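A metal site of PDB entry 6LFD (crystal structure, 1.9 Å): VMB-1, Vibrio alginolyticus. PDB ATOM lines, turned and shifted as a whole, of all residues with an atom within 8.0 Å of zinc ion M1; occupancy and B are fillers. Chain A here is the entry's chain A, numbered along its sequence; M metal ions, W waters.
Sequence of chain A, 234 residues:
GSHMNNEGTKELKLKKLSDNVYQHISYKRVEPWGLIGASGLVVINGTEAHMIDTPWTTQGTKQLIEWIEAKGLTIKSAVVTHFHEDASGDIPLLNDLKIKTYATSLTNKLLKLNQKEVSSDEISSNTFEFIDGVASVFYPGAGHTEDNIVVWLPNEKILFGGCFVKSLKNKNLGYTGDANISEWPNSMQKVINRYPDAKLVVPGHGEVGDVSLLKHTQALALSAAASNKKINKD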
ATOM      1  N   GLY A  37       8.930   8.471  -6.107  1.00  0.00           N
ATOM      2  CA  GLY A  37       8.215   8.908  -7.310  1.00  0.00           C
ATOM      3  C   GLY A  37       6.780   8.452  -7.423  1.00  0.00           C
ATOM      4  O   GLY A  37       6.387   7.502  -6.774  1.00  0.00           O
ATOM      5  N   ALA A  38       6.029   9.260  -8.152  1.00  0.00           N
ATOM      6  CA  ALA A  38       4.664   8.977  -8.620  1.00  0.00           C
ATOM      7  C   ALA A  38       4.742   8.953 -10.144  1.00  0.00           C
ATOM      8  O   ALA A  38       5.555   9.727 -10.725  1.00  0.00           O
ATOM      9  CB  ALA A  38       3.704  10.020  -8.113  1.00  0.00           C
ATOM     10  N   SER A  39       4.006   8.032 -10.763  1.00  0.00           N
ATOM     11  CA  SER A  39       3.979   7.825 -12.228  1.00  0.00           C
ATOM     12  C   SER A  39       2.633   8.260 -12.803  1.00  0.00           C
ATOM     13  O   SER A  39       1.595   7.972 -12.213  1.00  0.00           O
ATOM     14  CB  SER A  39       4.265   6.380 -12.581  1.00  0.00           C
ATOM     15  OG  SER A  39       5.619   6.078 -12.353  1.00  0.00           O
ATOM     16  N   ASP A  53      -2.925  11.349 -15.228  1.00  0.00           N
ATOM     17  CA  ASP A  53      -2.513  11.827 -13.878  1.00  0.00           C
ATOM     18  C   ASP A  53      -1.659  13.097 -14.023  1.00  0.00           C
ATOM     19  O   ASP A  53      -0.930  13.213 -15.037  1.00  0.00           O
ATOM     20  CB  ASP A  53      -1.775  10.739 -13.094  1.00  0.00           C
ATOM     21  CG  ASP A  53      -2.703   9.769 -12.380  1.00  0.00           C
ATOM     22  OD1 ASP A  53      -3.935   9.875 -12.575  1.00  0.00           O
ATOM     23  OD2 ASP A  53      -2.179   8.927 -11.640  1.00  0.00           O
ATOM     24  N   TRP A  56       3.102  15.075  -9.106  1.00  0.00           N
ATOM     25  CA  TRP A  56       2.867  15.103  -7.641  1.00  0.00           C
ATOM     26  C   TRP A  56       3.035  16.518  -7.080  1.00  0.00           C
ATOM     27  O   TRP A  56       2.443  16.819  -6.031  1.00  0.00           O
ATOM     28  CB  TRP A  56       3.834  14.124  -6.965  1.00  0.00           C
ATOM     29  CG  TRP A  56       3.325  13.482  -5.713  1.00  0.00           C
ATOM     30  CD1 TRP A  56       2.247  13.845  -4.946  1.00  0.00           C
ATOM     31  CD2 TRP A  56       3.930  12.352  -5.068  1.00  0.00           C
ATOM     32  NE1 TRP A  56       2.134  12.991  -3.875  1.00  0.00           N
ATOM     33  CE2 TRP A  56       3.157  12.081  -3.918  1.00  0.00           C
ATOM     34  CE3 TRP A  56       5.041  11.557  -5.357  1.00  0.00           C
ATOM     35  CZ2 TRP A  56       3.451  11.013  -3.079  1.00  0.00           C
ATOM     36  CZ3 TRP A  56       5.343  10.507  -4.507  1.00  0.00           C
ATOM     37  CH2 TRP A  56       4.554  10.245  -3.389  1.00  0.00           C
ATOM     38  N   HIS A  82      -7.463   9.043  -9.730  1.00  0.00           N
ATOM     39  CA  HIS A  82      -8.144   9.114  -8.420  1.00  0.00           C
ATOM     40  C   HIS A  82      -7.944  10.492  -7.794  1.00  0.00           C
ATOM     41  O   HIS A  82      -7.173  11.309  -8.342  1.00  0.00           O
ATOM     42  CB  HIS A  82      -7.741   7.934  -7.511  1.00  0.00           C
ATOM     43  CG  HIS A  82      -6.371   8.003  -6.925  1.00  0.00           C
ATOM     44  ND1 HIS A  82      -5.207   7.862  -7.667  1.00  0.00           N
ATOM     45  CD2 HIS A  82      -5.991   8.045  -5.626  1.00  0.00           C
ATOM     46  CE1 HIS A  82      -4.167   7.851  -6.826  1.00  0.00           C
ATOM     47  NE2 HIS A  82      -4.638   7.955  -5.576  1.00  0.00           N
ATOM     48  N   HIS A  84      -6.536  11.604  -4.988  1.00  0.00           N
ATOM     49  CA  HIS A  84      -5.306  11.972  -4.211  1.00  0.00           C
ATOM     50  C   HIS A  84      -4.411  12.907  -5.036  1.00  0.00           C
ATOM     51  O   HIS A  84      -4.505  12.891  -6.267  1.00  0.00           O
ATOM     52  CB  HIS A  84      -4.492  10.755  -3.787  1.00  0.00           C
ATOM     53  CG  HIS A  84      -5.166   9.900  -2.755  1.00  0.00           C
ATOM     54  ND1 HIS A  84      -4.843   8.574  -2.567  1.00  0.00           N
ATOM     55  CD2 HIS A  84      -6.147  10.187  -1.869  1.00  0.00           C
ATOM     56  CE1 HIS A  84      -5.596   8.097  -1.587  1.00  0.00           C
ATOM     57  NE2 HIS A  84      -6.419   9.060  -1.187  1.00  0.00           N
ATOM     58  N   GLU A  85      -3.545  13.641  -4.340  1.00  0.00           N
ATOM     59  CA  GLU A  85      -2.696  14.739  -4.909  1.00  0.00           C
ATOM     60  C   GLU A  85      -1.715  14.200  -5.967  1.00  0.00           C
ATOM     61  O   GLU A  85      -1.283  14.994  -6.851  1.00  0.00           O
ATOM     62  CB  GLU A  85      -1.917  15.414  -3.769  1.00  0.00           C
ATOM     63  CG  GLU A  85      -2.795  16.208  -2.815  1.00  0.00           C
ATOM     64  CD  GLU A  85      -2.996  17.690  -3.130  1.00  0.00           C
ATOM     65  OE1 GLU A  85      -2.101  18.293  -3.771  1.00  0.00           O
ATOM     66  OE2 GLU A  85      -4.046  18.254  -2.725  1.00  0.00           O
ATOM     67  N   ASP A  86      -1.348  12.925  -5.910  1.00  0.00           N
ATOM     68  CA  ASP A  86      -0.400  12.337  -6.902  1.00  0.00           C
ATOM     69  C   ASP A  86      -1.122  11.983  -8.221  1.00  0.00           C
ATOM     70  O   ASP A  86      -0.447  11.531  -9.155  1.00  0.00           O
ATOM     71  CB  ASP A  86       0.372  11.170  -6.312  1.00  0.00           C
ATOM     72  CG  ASP A  86      -0.502  10.051  -5.802  1.00  0.00           C
ATOM     73  OD1 ASP A  86      -1.637  10.322  -5.379  1.00  0.00           O
ATOM     74  OD2 ASP A  86      -0.047   8.944  -5.868  1.00  0.00           O
ATOM     75  N   ALA A  87      -2.435  12.192  -8.328  1.00  0.00           N
ATOM     76  CA  ALA A  87      -3.196  11.979  -9.578  1.00  0.00           C
ATOM     77  C   ALA A  87      -3.918  13.248  -9.995  1.00  0.00           C
ATOM     78  O   ALA A  87      -4.039  13.499 -11.206  1.00  0.00           O
ATOM     79  CB  ALA A  87      -4.174  10.833  -9.385  1.00  0.00           C
ATOM     80  N   HIS A 144      -7.819   0.914  -3.875  1.00  0.00           N
ATOM     81  CA  HIS A 144      -7.017   1.975  -3.229  1.00  0.00           C
ATOM     82  C   HIS A 144      -7.915   3.126  -2.758  1.00  0.00           C
ATOM     83  O   HIS A 144      -7.669   3.661  -1.650  1.00  0.00           O
ATOM     84  CB  HIS A 144      -5.903   2.417  -4.186  1.00  0.00           C
ATOM     85  CG  HIS A 144      -5.172   3.620  -3.712  1.00  0.00           C
ATOM     86  ND1 HIS A 144      -4.368   3.601  -2.587  1.00  0.00           N
ATOM     87  CD2 HIS A 144      -5.126   4.879  -4.207  1.00  0.00           C
ATOM     88  CE1 HIS A 144      -3.841   4.800  -2.420  1.00  0.00           C
ATOM     89  NE2 HIS A 144      -4.270   5.589  -3.403  1.00  0.00           N
ATOM     90  N   GLY A 162      -2.421   2.912 -12.159  1.00  0.00           N
ATOM     91  CA  GLY A 162      -2.275   3.925 -11.103  1.00  0.00           C
ATOM     92  C   GLY A 162      -2.141   3.277  -9.722  1.00  0.00           C
ATOM     93  O   GLY A 162      -1.673   2.160  -9.628  1.00  0.00           O
ATOM     94  N   CYS A 163      -2.613   3.942  -8.684  1.00  0.00           N
ATOM     95  CA  CYS A 163      -2.399   3.498  -7.288  1.00  0.00           C
ATOM     96  C   CYS A 163      -3.357   2.354  -6.933  1.00  0.00           C
ATOM     97  O   CYS A 163      -3.186   1.732  -5.853  1.00  0.00           O
ATOM     98  CB  CYS A 163      -2.443   4.700  -6.373  1.00  0.00           C
ATOM     99  SG  CYS A 163      -1.297   5.964  -6.971  1.00  0.00           S
ATOM    100  N   PHE A 164      -4.274   2.008  -7.842  1.00  0.00           N
ATOM    101  CA  PHE A 164      -5.067   0.751  -7.787  1.00  0.00           C
ATOM    102  C   PHE A 164      -4.156  -0.493  -7.918  1.00  0.00           C
ATOM    103  O   PHE A 164      -4.522  -1.627  -7.470  1.00  0.00           O
ATOM    104  CB  PHE A 164      -6.126   0.794  -8.894  1.00  0.00           C
ATOM    105  CG  PHE A 164      -7.037  -0.404  -8.943  1.00  0.00           C
ATOM    106  CD1 PHE A 164      -8.001  -0.598  -7.960  1.00  0.00           C
ATOM    107  CD2 PHE A 164      -6.955  -1.306  -9.981  1.00  0.00           C
ATOM    108  CE1 PHE A 164      -8.862  -1.681  -8.013  1.00  0.00           C
ATOM    109  CE2 PHE A 164      -7.802  -2.401 -10.026  1.00  0.00           C
ATOM    110  CZ  PHE A 164      -8.766  -2.565  -9.053  1.00  0.00           C
ATOM    111  N   VAL A 165      -2.985  -0.316  -8.529  1.00  0.00           N
ATOM    112  CA  VAL A 165      -2.028  -1.450  -8.762  1.00  0.00           C
ATOM    113  C   VAL A 165      -0.736  -1.141  -8.005  1.00  0.00           C
ATOM    114  O   VAL A 165      -0.234  -0.012  -8.087  1.00  0.00           O
ATOM    115  CB  VAL A 165      -1.780  -1.693 -10.274  1.00  0.00           C
ATOM    116  CG1 VAL A 165      -0.852  -2.861 -10.504  1.00  0.00           C
ATOM    117  CG2 VAL A 165      -3.086  -1.910 -11.026  1.00  0.00           C
ATOM    118  N   LYS A 166      -0.240  -2.121  -7.257  1.00  0.00           N
ATOM    119  CA  LYS A 166       1.052  -2.060  -6.496  1.00  0.00           C
ATOM    120  C   LYS A 166       2.168  -2.687  -7.350  1.00  0.00           C
ATOM    121  O   LYS A 166       1.871  -3.588  -8.131  1.00  0.00           O
ATOM    122  CB  LYS A 166       0.879  -2.803  -5.167  1.00  0.00           C
ATOM    123  CG  LYS A 166      -0.170  -2.241  -4.226  1.00  0.00           C
ATOM    124  CD  LYS A 166      -0.093  -0.738  -3.998  1.00  0.00           C
ATOM    125  CE  LYS A 166       1.010  -0.343  -3.033  1.00  0.00           C
ATOM    126  NZ  LYS A 166       1.073   1.130  -2.819  1.00  0.00           N
ATOM    127  N   TYR A 175      -0.929   3.464   1.632  1.00  0.00           N
ATOM    128  CA  TYR A 175      -1.921   4.254   2.391  1.00  0.00           C
ATOM    129  C   TYR A 175      -3.308   3.680   2.102  1.00  0.00           C
ATOM    130  O   TYR A 175      -3.683   3.696   0.922  1.00  0.00           O
ATOM    131  CB  TYR A 175      -1.819   5.728   2.043  1.00  0.00           C
ATOM    132  CG  TYR A 175      -2.909   6.546   2.670  1.00  0.00           C
ATOM    133  CD1 TYR A 175      -2.873   6.874   4.014  1.00  0.00           C
ATOM    134  CD2 TYR A 175      -4.000   6.961   1.934  1.00  0.00           C
ATOM    135  CE1 TYR A 175      -3.865   7.615   4.608  1.00  0.00           C
ATOM    136  CE2 TYR A 175      -5.007   7.724   2.511  1.00  0.00           C
ATOM    137  CZ  TYR A 175      -4.943   8.052   3.854  1.00  0.00           C
ATOM    138  OH  TYR A 175      -5.936   8.769   4.441  1.00  0.00           O
ATOM    139  N   PRO A 203       2.205   0.816 -12.420  1.00  0.00           N
ATOM    140  CA  PRO A 203       1.667   1.137 -11.096  1.00  0.00           C
ATOM    141  C   PRO A 203       1.818   2.632 -10.789  1.00  0.00           C
ATOM    142  O   PRO A 203       2.556   3.344 -11.469  1.00  0.00           O
ATOM    143  CB  PRO A 203       2.496   0.229 -10.177  1.00  0.00           C
ATOM    144  CG  PRO A 203       3.846   0.089 -10.878  1.00  0.00           C
ATOM    145  CD  PRO A 203       3.573   0.252 -12.355  1.00  0.00           C
ATOM    146  N   GLY A 204       1.068   3.127  -9.808  1.00  0.00           N
ATOM    147  CA  GLY A 204       1.094   4.556  -9.443  1.00  0.00           C
ATOM    148  C   GLY A 204       2.463   4.907  -8.888  1.00  0.00           C
ATOM    149  O   GLY A 204       2.897   6.036  -9.070  1.00  0.00           O
ATOM    150  N   HIS A 205       3.109   3.914  -8.277  1.00  0.00           N
ATOM    151  CA  HIS A 205       4.465   3.990  -7.658  1.00  0.00           C
ATOM    152  C   HIS A 205       5.209   2.677  -7.906  1.00  0.00           C
ATOM    153  O   HIS A 205       4.567   1.591  -7.788  1.00  0.00           O
ATOM    154  CB  HIS A 205       4.374   4.246  -6.137  1.00  0.00           C
ATOM    155  CG  HIS A 205       3.374   5.278  -5.746  1.00  0.00           C
ATOM    156  ND1 HIS A 205       3.691   6.632  -5.704  1.00  0.00           N
ATOM    157  CD2 HIS A 205       2.080   5.181  -5.372  1.00  0.00           C
ATOM    158  CE1 HIS A 205       2.633   7.312  -5.301  1.00  0.00           C
ATOM    159  NE2 HIS A 205       1.627   6.443  -5.121  1.00  0.00           N
HETATM  160 ZN    ZN M   1      -0.404   7.118  -5.156  1.00  0.00          ZN
HETATM  161 ZN    ZN M   2      -3.754   7.504  -3.709  1.00  0.00          ZN
HETATM  162  O   HOH W   1      -1.589   7.433  -3.379  1.00  0.00           O
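Zinc ion M1 is bound by OD2 of Asp 86 (2.0 Å), NE2 of His 205 (2.1 Å), water W1 (2.2 Å) and SG of Cys 163 (2.3 Å).
Within 4 Å of zinc ion M1: Asp 86, Cys 163 and His 205.
O of Gly 37 sits at hydrogen-bond distance from ND1 of His 205 (3.0 Å).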
